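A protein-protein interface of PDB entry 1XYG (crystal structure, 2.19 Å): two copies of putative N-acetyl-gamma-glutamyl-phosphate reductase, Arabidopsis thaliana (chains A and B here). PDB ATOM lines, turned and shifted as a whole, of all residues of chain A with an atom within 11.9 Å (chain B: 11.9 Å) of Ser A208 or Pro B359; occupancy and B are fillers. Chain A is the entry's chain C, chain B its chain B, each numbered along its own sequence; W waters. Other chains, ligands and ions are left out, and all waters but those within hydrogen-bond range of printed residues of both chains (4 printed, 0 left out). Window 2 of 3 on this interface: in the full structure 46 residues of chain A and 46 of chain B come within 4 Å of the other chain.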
ATOM      1  N   VAL A 194     -23.975 -28.473 -19.470  1.00  0.00           N
ATOM      2  CA  VAL A 194     -25.389 -28.417 -19.803  1.00  0.00           C
ATOM      3  C   VAL A 194     -25.718 -28.098 -21.271  1.00  0.00           C
ATOM      4  O   VAL A 194     -26.857 -28.250 -21.691  1.00  0.00           O
ATOM      5  CB  VAL A 194     -26.117 -27.433 -18.846  1.00  0.00           C
ATOM      6  CG1 VAL A 194     -25.621 -26.024 -19.070  1.00  0.00           C
ATOM      7  CG2 VAL A 194     -27.630 -27.547 -19.018  1.00  0.00           C
ATOM      8  N   LYS A 202     -36.507 -25.060 -21.220  1.00  0.00           N
ATOM      9  CA  LYS A 202     -37.048 -25.823 -20.103  1.00  0.00           C
ATOM     10  C   LYS A 202     -36.581 -25.316 -18.738  1.00  0.00           C
ATOM     11  O   LYS A 202     -35.421 -24.939 -18.547  1.00  0.00           O
ATOM     12  CB  LYS A 202     -36.741 -27.312 -20.273  1.00  0.00           C
ATOM     13  CG  LYS A 202     -35.410 -27.618 -20.884  1.00  0.00           C
ATOM     14  CD  LYS A 202     -35.420 -28.981 -21.567  1.00  0.00           C
ATOM     15  CE  LYS A 202     -35.794 -28.855 -23.035  1.00  0.00           C
ATOM     16  NZ  LYS A 202     -35.682 -30.156 -23.756  1.00  0.00           N
ATOM     17  N   GLU A 203     -37.515 -25.314 -17.793  1.00  0.00           N
ATOM     18  CA  GLU A 203     -37.263 -24.845 -16.440  1.00  0.00           C
ATOM     19  C   GLU A 203     -36.002 -25.447 -15.828  1.00  0.00           C
ATOM     20  O   GLU A 203     -35.170 -24.740 -15.252  1.00  0.00           O
ATOM     21  CB  GLU A 203     -38.456 -25.178 -15.550  1.00  0.00           C
ATOM     22  CG  GLU A 203     -38.386 -24.530 -14.195  1.00  0.00           C
ATOM     23  CD  GLU A 203     -39.450 -25.049 -13.257  1.00  0.00           C
ATOM     24  OE1 GLU A 203     -39.250 -26.142 -12.684  1.00  0.00           O
ATOM     25  OE2 GLU A 203     -40.488 -24.367 -13.104  1.00  0.00           O
ATOM     26  N   ALA A 204     -35.860 -26.758 -15.963  1.00  0.00           N
ATOM     27  CA  ALA A 204     -34.717 -27.455 -15.394  1.00  0.00           C
ATOM     28  C   ALA A 204     -33.354 -26.953 -15.858  1.00  0.00           C
ATOM     29  O   ALA A 204     -32.370 -27.100 -15.134  1.00  0.00           O
ATOM     30  CB  ALA A 204     -34.834 -28.939 -15.669  1.00  0.00           C
ATOM     31  N   ASN A 205     -33.284 -26.355 -17.043  1.00  0.00           N
ATOM     32  CA  ASN A 205     -32.001 -25.880 -17.548  1.00  0.00           C
ATOM     33  C   ASN A 205     -31.725 -24.384 -17.436  1.00  0.00           C
ATOM     34  O   ASN A 205     -30.787 -23.878 -18.051  1.00  0.00           O
ATOM     35  CB  ASN A 205     -31.811 -26.356 -18.987  1.00  0.00           C
ATOM     36  CG  ASN A 205     -31.763 -27.878 -19.083  1.00  0.00           C
ATOM     37  OD1 ASN A 205     -31.278 -28.551 -18.165  1.00  0.00           O
ATOM     38  ND2 ASN A 205     -32.258 -28.428 -20.196  1.00  0.00           N
ATOM     39  N   LEU A 206     -32.534 -23.682 -16.649  1.00  0.00           N
ATOM     40  CA  LEU A 206     -32.339 -22.255 -16.439  1.00  0.00           C
ATOM     41  C   LEU A 206     -31.048 -22.068 -15.639  1.00  0.00           C
ATOM     42  O   LEU A 206     -30.633 -22.965 -14.892  1.00  0.00           O
ATOM     43  CB  LEU A 206     -33.505 -21.668 -15.638  1.00  0.00           C
ATOM     44  CG  LEU A 206     -34.873 -21.574 -16.317  1.00  0.00           C
ATOM     45  CD1 LEU A 206     -35.934 -21.130 -15.302  1.00  0.00           C
ATOM     46  CD2 LEU A 206     -34.780 -20.594 -17.476  1.00  0.00           C
ATOM     47  N   TYR A 207     -30.414 -20.908 -15.794  1.00  0.00           N
ATOM     48  CA  TYR A 207     -29.188 -20.620 -15.064  1.00  0.00           C
ATOM     49  C   TYR A 207     -29.400 -20.793 -13.553  1.00  0.00           C
ATOM     50  O   TYR A 207     -28.595 -21.439 -12.876  1.00  0.00           O
ATOM     51  CB  TYR A 207     -28.707 -19.188 -15.358  1.00  0.00           C
ATOM     52  CG  TYR A 207     -27.390 -18.853 -14.689  1.00  0.00           C
ATOM     53  CD1 TYR A 207     -27.344 -18.405 -13.368  1.00  0.00           C
ATOM     54  CD2 TYR A 207     -26.183 -19.097 -15.343  1.00  0.00           C
ATOM     55  CE1 TYR A 207     -26.123 -18.220 -12.706  1.00  0.00           C
ATOM     56  CE2 TYR A 207     -24.959 -18.923 -14.698  1.00  0.00           C
ATOM     57  CZ  TYR A 207     -24.931 -18.490 -13.375  1.00  0.00           C
ATOM     58  OH  TYR A 207     -23.719 -18.378 -12.721  1.00  0.00           O
ATOM     59  N   SER A 208     -30.488 -20.224 -13.039  1.00  0.00           N
ATOM     60  CA  SER A 208     -30.800 -20.296 -11.614  1.00  0.00           C
ATOM     61  C   SER A 208     -31.010 -21.713 -11.076  1.00  0.00           C
ATOM     62  O   SER A 208     -30.860 -21.950  -9.876  1.00  0.00           O
ATOM     63  CB  SER A 208     -32.047 -19.462 -11.296  1.00  0.00           C
ATOM     64  OG  SER A 208     -31.863 -18.100 -11.630  1.00  0.00           O
ATOM     65  N   GLU A 209     -31.377 -22.646 -11.948  1.00  0.00           N
ATOM     66  CA  GLU A 209     -31.610 -24.024 -11.532  1.00  0.00           C
ATOM     67  C   GLU A 209     -30.354 -24.884 -11.663  1.00  0.00           C
ATOM     68  O   GLU A 209     -30.146 -25.812 -10.887  1.00  0.00           O
ATOM     69  CB  GLU A 209     -32.726 -24.658 -12.379  1.00  0.00           C
ATOM     70  CG  GLU A 209     -34.104 -23.994 -12.292  1.00  0.00           C
ATOM     71  CD  GLU A 209     -34.804 -24.244 -10.972  1.00  0.00           C
ATOM     72  OE1 GLU A 209     -34.841 -25.406 -10.528  1.00  0.00           O
ATOM     73  OE2 GLU A 209     -35.331 -23.284 -10.383  1.00  0.00           O
ATOM     74  N   ILE A 210     -29.521 -24.572 -12.654  1.00  0.00           N
ATOM     75  CA  ILE A 210     -28.313 -25.345 -12.915  1.00  0.00           C
ATOM     76  C   ILE A 210     -27.070 -24.906 -12.146  1.00  0.00           C
ATOM     77  O   ILE A 210     -26.348 -25.735 -11.597  1.00  0.00           O
ATOM     78  CB  ILE A 210     -27.973 -25.310 -14.426  1.00  0.00           C
ATOM     79  CG1 ILE A 210     -29.066 -26.036 -15.227  1.00  0.00           C
ATOM     80  CG2 ILE A 210     -26.567 -25.883 -14.678  1.00  0.00           C
ATOM     81  CD1 ILE A 210     -29.178 -27.525 -14.952  1.00  0.00           C
ATOM     82  N   ALA A 211     -26.822 -23.603 -12.117  1.00  0.00           N
ATOM     83  CA  ALA A 211     -25.633 -23.052 -11.471  1.00  0.00           C
ATOM     84  C   ALA A 211     -25.376 -23.445 -10.024  1.00  0.00           C
ATOM     85  O   ALA A 211     -26.306 -23.602  -9.224  1.00  0.00           O
ATOM     86  CB  ALA A 211     -25.643 -21.539 -11.588  1.00  0.00           C
ATOM     87  N   GLU A 212     -24.089 -23.605  -9.709  1.00  0.00           N
ATOM     88  CA  GLU A 212     -23.633 -23.931  -8.364  1.00  0.00           C
ATOM     89  C   GLU A 212     -24.135 -25.241  -7.782  1.00  0.00           C
ATOM     90  O   GLU A 212     -24.485 -25.309  -6.602  1.00  0.00           O
ATOM     91  CB  GLU A 212     -23.982 -22.780  -7.415  1.00  0.00           C
ATOM     92  CG  GLU A 212     -23.173 -21.513  -7.670  1.00  0.00           C
ATOM     93  CD  GLU A 212     -21.672 -21.741  -7.525  1.00  0.00           C
ATOM     94  OE1 GLU A 212     -21.261 -22.271  -6.475  1.00  0.00           O
ATOM     95  OE2 GLU A 212     -20.904 -21.389  -8.456  1.00  0.00           O
ATOM     96  N   GLY A 213     -24.149 -26.281  -8.606  1.00  0.00           N
ATOM     97  CA  GLY A 213     -24.583 -27.580  -8.146  1.00  0.00           C
ATOM     98  C   GLY A 213     -24.519 -28.609  -9.252  1.00  0.00           C
ATOM     99  O   GLY A 213     -24.401 -28.262 -10.428  1.00  0.00           O
ATOM    100  N   ILE A 214     -24.583 -29.879  -8.874  1.00  0.00           N
ATOM    101  CA  ILE A 214     -24.569 -30.961  -9.850  1.00  0.00           C
ATOM    102  C   ILE A 214     -25.630 -31.984  -9.465  1.00  0.00           C
ATOM    103  O   ILE A 214     -26.206 -31.920  -8.368  1.00  0.00           O
ATOM    104  CB  ILE A 214     -23.203 -31.702  -9.917  1.00  0.00           C
ATOM    105  CG1 ILE A 214     -22.894 -32.387  -8.581  1.00  0.00           C
ATOM    106  CG2 ILE A 214     -22.101 -30.738 -10.327  1.00  0.00           C
ATOM    107  CD1 ILE A 214     -21.798 -33.444  -8.684  1.00  0.00           C
ATOM    108  N   SER A 215     -25.885 -32.913 -10.375  1.00  0.00           N
ATOM    109  CA  SER A 215     -26.847 -33.982 -10.151  1.00  0.00           C
ATOM    110  C   SER A 215     -26.677 -35.029 -11.233  1.00  0.00           C
ATOM    111  O   SER A 215     -26.187 -34.728 -12.323  1.00  0.00           O
ATOM    112  CB  SER A 215     -28.288 -33.450 -10.175  1.00  0.00           C
ATOM    113  OG  SER A 215     -28.637 -32.873 -11.423  1.00  0.00           O
ATOM    114  N   LEU A 248     -24.875 -33.951 -14.640  1.00  0.00           N
ATOM    115  CA  LEU A 248     -24.978 -32.622 -15.238  1.00  0.00           C
ATOM    116  C   LEU A 248     -24.098 -31.616 -14.498  1.00  0.00           C
ATOM    117  O   LEU A 248     -24.278 -31.391 -13.301  1.00  0.00           O
ATOM    118  CB  LEU A 248     -26.436 -32.155 -15.219  1.00  0.00           C
ATOM    119  CG  LEU A 248     -26.795 -31.004 -16.163  1.00  0.00           C
ATOM    120  CD1 LEU A 248     -26.477 -31.405 -17.590  1.00  0.00           C
ATOM    121  CD2 LEU A 248     -28.268 -30.671 -16.034  1.00  0.00           C
ATOM    122  N   MET A 249     -23.155 -31.016 -15.227  1.00  0.00           N
ATOM    123  CA  MET A 249     -22.215 -30.047 -14.670  1.00  0.00           C
ATOM    124  C   MET A 249     -22.637 -28.589 -14.854  1.00  0.00           C
ATOM    125  O   MET A 249     -23.190 -28.219 -15.892  1.00  0.00           O
ATOM    126  CB  MET A 249     -20.837 -30.222 -15.322  1.00  0.00           C
ATOM    127  CG  MET A 249     -20.220 -31.610 -15.201  1.00  0.00           C
ATOM    128  SD  MET A 249     -19.794 -32.027 -13.497  1.00  0.00           S
ATOM    129  CE  MET A 249     -21.244 -32.987 -13.025  1.00  0.00           C
ATOM    130  N   PRO A 250     -22.363 -27.735 -13.849  1.00  0.00           N
ATOM    131  CA  PRO A 250     -22.722 -26.322 -13.952  1.00  0.00           C
ATOM    132  C   PRO A 250     -21.671 -25.610 -14.806  1.00  0.00           C
ATOM    133  O   PRO A 250     -20.853 -24.833 -14.308  1.00  0.00           O
ATOM    134  CB  PRO A 250     -22.717 -25.865 -12.494  1.00  0.00           C
ATOM    135  CG  PRO A 250     -21.580 -26.647 -11.935  1.00  0.00           C
ATOM    136  CD  PRO A 250     -21.790 -28.026 -12.521  1.00  0.00           C
ATOM    137  N   MET A 251     -21.688 -25.914 -16.097  1.00  0.00           N
ATOM    138  CA  MET A 251     -20.772 -25.324 -17.067  1.00  0.00           C
ATOM    139  C   MET A 251     -21.407 -25.529 -18.438  1.00  0.00           C
ATOM    140  O   MET A 251     -22.269 -26.392 -18.606  1.00  0.00           O
ATOM    141  CB  MET A 251     -19.401 -26.009 -17.011  1.00  0.00           C
ATOM    142  CG  MET A 251     -19.434 -27.502 -17.341  1.00  0.00           C
ATOM    143  SD  MET A 251     -17.885 -28.320 -16.888  1.00  0.00           S
ATOM    144  CE  MET A 251     -17.973 -29.854 -17.839  1.00  0.00           C
ATOM    145  N   ILE A 252     -20.977 -24.740 -19.414  1.00  0.00           N
ATOM    146  CA  ILE A 252     -21.533 -24.831 -20.754  1.00  0.00           C
ATOM    147  C   ILE A 252     -20.998 -26.013 -21.550  1.00  0.00           C
ATOM    148  O   ILE A 252     -21.751 -26.904 -21.934  1.00  0.00           O
ATOM    149  CB  ILE A 252     -21.255 -23.535 -21.561  1.00  0.00           C
ATOM    150  CG1 ILE A 252     -21.836 -22.326 -20.828  1.00  0.00           C
ATOM    151  CG2 ILE A 252     -21.846 -23.650 -22.970  1.00  0.00           C
ATOM    152  CD1 ILE A 252     -21.565 -21.011 -21.532  1.00  0.00           C
ATOM    153  N   MET B 251     -17.896 -24.864  -8.997  1.00  0.00           N
ATOM    154  CA  MET B 251     -18.935 -24.322  -8.124  1.00  0.00           C
ATOM    155  C   MET B 251     -18.296 -24.153  -6.746  1.00  0.00           C
ATOM    156  O   MET B 251     -17.274 -24.778  -6.448  1.00  0.00           O
ATOM    157  CB  MET B 251     -20.134 -25.280  -8.035  1.00  0.00           C
ATOM    158  CG  MET B 251     -19.816 -26.646  -7.432  1.00  0.00           C
ATOM    159  SD  MET B 251     -21.097 -27.876  -7.737  1.00  0.00           S
ATOM    160  CE  MET B 251     -20.803 -29.064  -6.371  1.00  0.00           C
ATOM    161  N   ILE B 252     -18.896 -23.312  -5.917  1.00  0.00           N
ATOM    162  CA  ILE B 252     -18.356 -23.054  -4.591  1.00  0.00           C
ATOM    163  C   ILE B 252     -18.642 -24.157  -3.582  1.00  0.00           C
ATOM    164  O   ILE B 252     -17.714 -24.784  -3.064  1.00  0.00           O
ATOM    165  CB  ILE B 252     -18.892 -21.739  -4.013  1.00  0.00           C
ATOM    166  CG1 ILE B 252     -18.615 -20.591  -4.984  1.00  0.00           C
ATOM    167  CG2 ILE B 252     -18.232 -21.469  -2.659  1.00  0.00           C
ATOM    168  CD1 ILE B 252     -19.180 -19.272  -4.519  1.00  0.00           C
ATOM    169  N   ARG B 253     -19.928 -24.387  -3.317  1.00  0.00           N
ATOM    170  CA  ARG B 253     -20.363 -25.395  -2.352  1.00  0.00           C
ATOM    171  C   ARG B 253     -21.024 -26.590  -3.020  1.00  0.00           C
ATOM    172  O   ARG B 253     -21.480 -26.503  -4.162  1.00  0.00           O
ATOM    173  CB  ARG B 253     -21.370 -24.786  -1.373  1.00  0.00           C
ATOM    174  CG  ARG B 253     -20.868 -23.591  -0.609  1.00  0.00           C
ATOM    175  CD  ARG B 253     -21.974 -22.979   0.228  1.00  0.00           C
ATOM    176  NE  ARG B 253     -21.461 -21.921   1.087  1.00  0.00           N
ATOM    177  CZ  ARG B 253     -21.445 -21.979   2.416  1.00  0.00           C
ATOM    178  NH1 ARG B 253     -21.924 -23.053   3.041  1.00  0.00           N
ATOM    179  NH2 ARG B 253     -20.939 -20.968   3.120  1.00  0.00           N
ATOM    180  N   GLY B 254     -21.084 -27.704  -2.296  1.00  0.00           N
ATOM    181  CA  GLY B 254     -21.729 -28.883  -2.834  1.00  0.00           C
ATOM    182  C   GLY B 254     -20.828 -30.086  -2.976  1.00  0.00           C
ATOM    183  O   GLY B 254     -19.655 -29.984  -3.355  1.00  0.00           O
ATOM    184  N   ARG B 296     -30.033 -33.628  -5.588  1.00  0.00           N
ATOM    185  CA  ARG B 296     -29.253 -32.569  -6.229  1.00  0.00           C
ATOM    186  C   ARG B 296     -28.477 -31.815  -5.156  1.00  0.00           C
ATOM    187  O   ARG B 296     -29.047 -31.487  -4.123  1.00  0.00           O
ATOM    188  CB  ARG B 296     -30.196 -31.592  -6.957  1.00  0.00           C
ATOM    189  CG  ARG B 296     -30.192 -31.710  -8.477  1.00  0.00           C
ATOM    190  CD  ARG B 296     -31.461 -31.158  -9.155  1.00  0.00           C
ATOM    191  NE  ARG B 296     -31.797 -29.767  -8.838  1.00  0.00           N
ATOM    192  CZ  ARG B 296     -31.296 -28.695  -9.451  1.00  0.00           C
ATOM    193  NH1 ARG B 296     -30.408 -28.820 -10.427  1.00  0.00           N
ATOM    194  NH2 ARG B 296     -31.720 -27.488  -9.112  1.00  0.00           N
ATOM    195  N   THR B 297     -27.189 -31.545  -5.381  1.00  0.00           N
ATOM    196  CA  THR B 297     -26.418 -30.798  -4.385  1.00  0.00           C
ATOM    197  C   THR B 297     -27.054 -29.423  -4.199  1.00  0.00           C
ATOM    198  O   THR B 297     -26.938 -28.812  -3.129  1.00  0.00           O
ATOM    199  CB  THR B 297     -24.923 -30.614  -4.797  1.00  0.00           C
ATOM    200  OG1 THR B 297     -24.847 -29.826  -5.990  1.00  0.00           O
ATOM    201  CG2 THR B 297     -24.248 -31.973  -5.047  1.00  0.00           C
ATOM    202  N   HIS B 298     -27.726 -28.934  -5.239  1.00  0.00           N
ATOM    203  CA  HIS B 298     -28.393 -27.635  -5.161  1.00  0.00           C
ATOM    204  C   HIS B 298     -29.396 -27.626  -4.005  1.00  0.00           C
ATOM    205  O   HIS B 298     -29.598 -26.598  -3.361  1.00  0.00           O
ATOM    206  CB  HIS B 298     -29.181 -27.315  -6.445  1.00  0.00           C
ATOM    207  CG  HIS B 298     -28.437 -27.564  -7.724  1.00  0.00           C
ATOM    208  ND1 HIS B 298     -28.078 -28.827  -8.143  1.00  0.00           N
ATOM    209  CD2 HIS B 298     -28.064 -26.719  -8.716  1.00  0.00           C
ATOM    210  CE1 HIS B 298     -27.523 -28.751  -9.341  1.00  0.00           C
ATOM    211  NE2 HIS B 298     -27.503 -27.482  -9.713  1.00  0.00           N
ATOM    212  N   ASN B 299     -30.016 -28.775  -3.744  1.00  0.00           N
ATOM    213  CA  ASN B 299     -31.045 -28.884  -2.712  1.00  0.00           C
ATOM    214  C   ASN B 299     -30.624 -28.871  -1.250  1.00  0.00           C
ATOM    215  O   ASN B 299     -31.476 -28.730  -0.375  1.00  0.00           O
ATOM    216  CB  ASN B 299     -31.914 -30.123  -2.966  1.00  0.00           C
ATOM    217  CG  ASN B 299     -32.626 -30.071  -4.311  1.00  0.00           C
ATOM    218  OD1 ASN B 299     -33.048 -29.002  -4.755  1.00  0.00           O
ATOM    219  ND2 ASN B 299     -32.770 -31.222  -4.959  1.00  0.00           N
ATOM    220  N   VAL B 300     -29.331 -29.019  -0.976  1.00  0.00           N
ATOM    221  CA  VAL B 300     -28.845 -29.004   0.403  1.00  0.00           C
ATOM    222  C   VAL B 300     -27.866 -27.851   0.616  1.00  0.00           C
ATOM    223  O   VAL B 300     -27.360 -27.634   1.718  1.00  0.00           O
ATOM    224  CB  VAL B 300     -28.143 -30.339   0.773  1.00  0.00           C
ATOM    225  CG1 VAL B 300     -29.123 -31.494   0.634  1.00  0.00           C
ATOM    226  CG2 VAL B 300     -26.923 -30.574  -0.119  1.00  0.00           C
ATOM    227  N   ARG B 301     -27.619 -27.112  -0.458  1.00  0.00           N
ATOM    228  CA  ARG B 301     -26.709 -25.974  -0.452  1.00  0.00           C
ATOM    229  C   ARG B 301     -26.994 -25.001   0.690  1.00  0.00           C
ATOM    230  O   ARG B 301     -28.101 -24.473   0.807  1.00  0.00           O
ATOM    231  CB  ARG B 301     -26.813 -25.248  -1.800  1.00  0.00           C
ATOM    232  CG  ARG B 301     -25.664 -24.321  -2.115  1.00  0.00           C
ATOM    233  CD  ARG B 301     -25.667 -23.944  -3.593  1.00  0.00           C
ATOM    234  NE  ARG B 301     -26.874 -23.222  -3.990  1.00  0.00           N
ATOM    235  CZ  ARG B 301     -27.440 -23.332  -5.190  1.00  0.00           C
ATOM    236  NH1 ARG B 301     -26.911 -24.137  -6.101  1.00  0.00           N
ATOM    237  NH2 ARG B 301     -28.528 -22.637  -5.481  1.00  0.00           N
ATOM    238  N   GLY B 302     -25.991 -24.772   1.530  1.00  0.00           N
ATOM    239  CA  GLY B 302     -26.145 -23.849   2.639  1.00  0.00           C
ATOM    240  C   GLY B 302     -26.884 -24.398   3.849  1.00  0.00           C
ATOM    241  O   GLY B 302     -27.319 -23.638   4.712  1.00  0.00           O
ATOM    242  N   SER B 303     -27.033 -25.715   3.913  1.00  0.00           N
ATOM    243  CA  SER B 303     -27.722 -26.336   5.034  1.00  0.00           C
ATOM    244  C   SER B 303     -26.893 -27.506   5.540  1.00  0.00           C
ATOM    245  O   SER B 303     -25.883 -27.870   4.944  1.00  0.00           O
ATOM    246  CB  SER B 303     -29.104 -26.838   4.611  1.00  0.00           C
ATOM    247  OG  SER B 303     -28.990 -28.012   3.820  1.00  0.00           O
ATOM    248  N   ASP B 326     -23.619 -30.246   1.658  1.00  0.00           N
ATOM    249  CA  ASP B 326     -22.936 -28.984   1.412  1.00  0.00           C
ATOM    250  C   ASP B 326     -21.599 -29.331   2.090  1.00  0.00           C
ATOM    251  O   ASP B 326     -21.566 -29.559   3.300  1.00  0.00           O
ATOM    252  CB  ASP B 326     -23.638 -27.840   2.153  1.00  0.00           C
ATOM    253  CG  ASP B 326     -22.904 -26.521   2.018  1.00  0.00           C
ATOM    254  OD1 ASP B 326     -21.656 -26.557   2.016  1.00  0.00           O
ATOM    255  OD2 ASP B 326     -23.565 -25.457   1.924  1.00  0.00           O
ATOM    256  N   GLN B 355     -32.379 -23.455   6.437  1.00  0.00           N
ATOM    257  CA  GLN B 355     -32.905 -24.156   5.270  1.00  0.00           C
ATOM    258  C   GLN B 355     -32.040 -23.863   4.049  1.00  0.00           C
ATOM    259  O   GLN B 355     -31.429 -22.799   3.959  1.00  0.00           O
ATOM    260  CB  GLN B 355     -34.361 -23.754   5.020  1.00  0.00           C
ATOM    261  CG  GLN B 355     -35.312 -24.323   6.063  1.00  0.00           C
ATOM    262  CD  GLN B 355     -35.112 -25.818   6.249  1.00  0.00           C
ATOM    263  OE1 GLN B 355     -35.375 -26.607   5.341  1.00  0.00           O
ATOM    264  NE2 GLN B 355     -34.621 -26.214   7.422  1.00  0.00           N
ATOM    265  N   PRO B 356     -31.974 -24.808   3.093  1.00  0.00           N
ATOM    266  CA  PRO B 356     -31.164 -24.630   1.883  1.00  0.00           C
ATOM    267  C   PRO B 356     -31.395 -23.299   1.175  1.00  0.00           C
ATOM    268  O   PRO B 356     -32.534 -22.828   1.059  1.00  0.00           O
ATOM    269  CB  PRO B 356     -31.564 -25.824   1.019  1.00  0.00           C
ATOM    270  CG  PRO B 356     -31.846 -26.875   2.035  1.00  0.00           C
ATOM    271  CD  PRO B 356     -32.678 -26.099   3.052  1.00  0.00           C
ATOM    272  N   LEU B 357     -30.309 -22.693   0.714  1.00  0.00           N
ATOM    273  CA  LEU B 357     -30.415 -21.435   0.001  1.00  0.00           C
ATOM    274  C   LEU B 357     -30.529 -21.719  -1.499  1.00  0.00           C
ATOM    275  O   LEU B 357     -29.524 -21.766  -2.206  1.00  0.00           O
ATOM    276  CB  LEU B 357     -29.190 -20.552   0.271  1.00  0.00           C
ATOM    277  CG  LEU B 357     -29.372 -19.102  -0.183  1.00  0.00           C
ATOM    278  CD1 LEU B 357     -30.426 -18.427   0.712  1.00  0.00           C
ATOM    279  CD2 LEU B 357     -28.037 -18.369  -0.111  1.00  0.00           C
ATOM    280  N   PHE B 358     -31.757 -21.926  -1.964  1.00  0.00           N
ATOM    281  CA  PHE B 358     -32.001 -22.191  -3.359  1.00  0.00           C
ATOM    282  C   PHE B 358     -33.117 -21.293  -3.869  1.00  0.00           C
ATOM    283  O   PHE B 358     -34.108 -21.099  -3.217  1.00  0.00           O
ATOM    284  CB  PHE B 358     -32.363 -23.660  -3.605  1.00  0.00           C
ATOM    285  CG  PHE B 358     -32.691 -23.967  -5.043  1.00  0.00           C
ATOM    286  CD1 PHE B 358     -33.963 -23.692  -5.558  1.00  0.00           C
ATOM    287  CD2 PHE B 358     -31.716 -24.483  -5.900  1.00  0.00           C
ATOM    288  CE1 PHE B 358     -34.264 -23.927  -6.901  1.00  0.00           C
ATOM    289  CE2 PHE B 358     -32.017 -24.723  -7.264  1.00  0.00           C
ATOM    290  CZ  PHE B 358     -33.290 -24.439  -7.754  1.00  0.00           C
ATOM    291  N   PRO B 359     -32.924 -20.679  -5.049  1.00  0.00           N
ATOM    292  CA  PRO B 359     -31.728 -20.808  -5.899  1.00  0.00           C
ATOM    293  C   PRO B 359     -30.545 -19.995  -5.311  1.00  0.00           C
ATOM    294  O   PRO B 359     -30.758 -19.240  -4.348  1.00  0.00           O
ATOM    295  CB  PRO B 359     -32.234 -20.278  -7.221  1.00  0.00           C
ATOM    296  CG  PRO B 359     -33.135 -19.160  -6.824  1.00  0.00           C
ATOM    297  CD  PRO B 359     -33.893 -19.717  -5.655  1.00  0.00           C
ATOM    298  OXT PRO B 359     -29.432 -20.255  -5.811  1.00  0.00           O
HETATM  299  O   HOH W   1     -22.323 -23.327  -4.333  1.00  0.00           O
HETATM  300  O   HOH W   2     -24.152 -27.503  -4.869  1.00  0.00           O
HETATM  301  O   HOH W   3     -28.777 -23.330  -8.702  1.00  0.00           O
HETATM  302  O   HOH W   4     -28.766 -30.539 -12.069  1.00  0.00           O
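SD of Met B251 sits close to N of Gly A213.
The backbone NH (N) of Ile B252 lies within hydrogen-bond range of the side-chain carboxylate (OE1) of Glu A212, 2.6 Å away.
The backbone carbonyl oxygen of Glu A209 sits at hydrogen-bond distance from the guanidinium group of Arg B296, 2.9 Å away.
OG1 of Thr B297 sits at hydrogen-bond distance from N of Ile A214 (2.9 Å).
The backbone carbonyl oxygen (O) of Glu A209 lies close to a ring nitrogen (NE2) of His B298.
A ring nitrogen (NE2) of His B298 is in hydrogen-bond range of the backbone carbonyl oxygen (O) of Ile A210 (2.8 Å).
A ring nitrogen (NE2) of His B298 lies close to the backbone carbonyl oxygen (O) of Gly A213, at 3.3 Å.
NH1 of Arg B301 is in hydrogen-bond range of O of Ala A211, at 3.2 Å.
The backbone carbonyl oxygen of Glu A212 lies within hydrogen-bond range of the guanidinium group of Arg B301.
The guanidinium group of Arg B296 sits close to a ring nitrogen (ND1) of His B298 (3.3 Å).
The backbone NH (N) of Leu B357 lies within hydrogen-bond range of the backbone carbonyl oxygen (O) of Arg B301, at 2.8 Å.
OXT of Pro B359 is in salt-bridge range of NH2 of Arg B301, 2.6 Å away.
The backbone NH of Leu A248 sits at hydrogen-bond distance from the backbone carbonyl oxygen of Ser A215.
Among the printed residues, pairs that only touch across the chains: Ser A208 with Phe B358 (3.98 Å), Ser A208 with Pro B359 (3.4 Å), Glu A209 with Phe B358 (3.3 Å), Ala A211 with His B298 (3.6 Å), Glu A212 with Met B251 (3.5 Å), Gly A213 with Thr B297 (3.1 Å), Ile A214 with Met B251 (3.99 Å), Ile A214 with Arg B296 (3.8 Å), Ile A214 with His B298 (3.2 Å) and Ser A215 with Arg B296 (3.1 Å).
No residue of chain B comes within 4 Å of Leu A206.
No residue of chain B comes within 4 Å of Tyr A207.
Of the printed residues of chain B, Ser A208 touches Phe B358 (3.98 Å) and Pro B359 (3.4 Å).
Glu A209 touches just these residues of chain B: Arg B296 (2.9 Å), His B298 (3.1 Å) and Phe B358 (3.3 Å).
Printed residues of chain B within 4 Å of Ile A210: His B298 (2.8 Å).
Of the printed residues of chain B, Glu A212 touches Met B251 (3.5 Å), Ile B252 (2.6 Å) and Arg B301 (2.7 Å).
Printed residues of chain A within 4 Å of Ile B252: Glu A212.
Of the printed residues of chain A, Arg B301 touches Ala A211 (3.2 Å) and Glu A212 (2.7 Å).
No residue of chain A comes within 4 Å of Leu B357.
Pro B359 touches one residue of chain A.
The nearest printed residue of chain B that does not touch Ser A208 is Arg B301 (5.0 Å).
The nearest residue of chain A that does not touch Pro B359 is Glu A209 (5.4 Å).
Hydrophobic or aromatic side chains of chain B that line the printed part of chain A: Met B251, Ile B252, His B298, Phe B358 and Pro B359.
Among the printed residues, 19 pairs touch across the chains.
Among the printed residues, no Asp or Glu carboxylate lies within 4 Å of a Lys or Arg side-chain nitrogen of the other chain.
2 positions are printed for both chains.
Of the 19 pairs that touch across the chains among the printed residues, none has its exchanged pair printed and touching as well.
Water W3 lies within hydrogen-bond range of O of Ala A211 (2.5 Å), O of Ser A208 (2.8 Å) and NH1 of Arg B301 (3.3 Å).
Water W1 lies within hydrogen-bond range of the side-chain carboxylate (OE1) of Glu A212 and the backbone NH (N) of Arg B253.
Water W2 lies within hydrogen-bond range of the side-chain hydroxyl (OG1) of Thr B297 (2.7 Å), the backbone carbonyl oxygen (O) of Glu A212 (2.8 Å) and the backbone carbonyl oxygen (O) of Arg B253 (2.9 Å).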
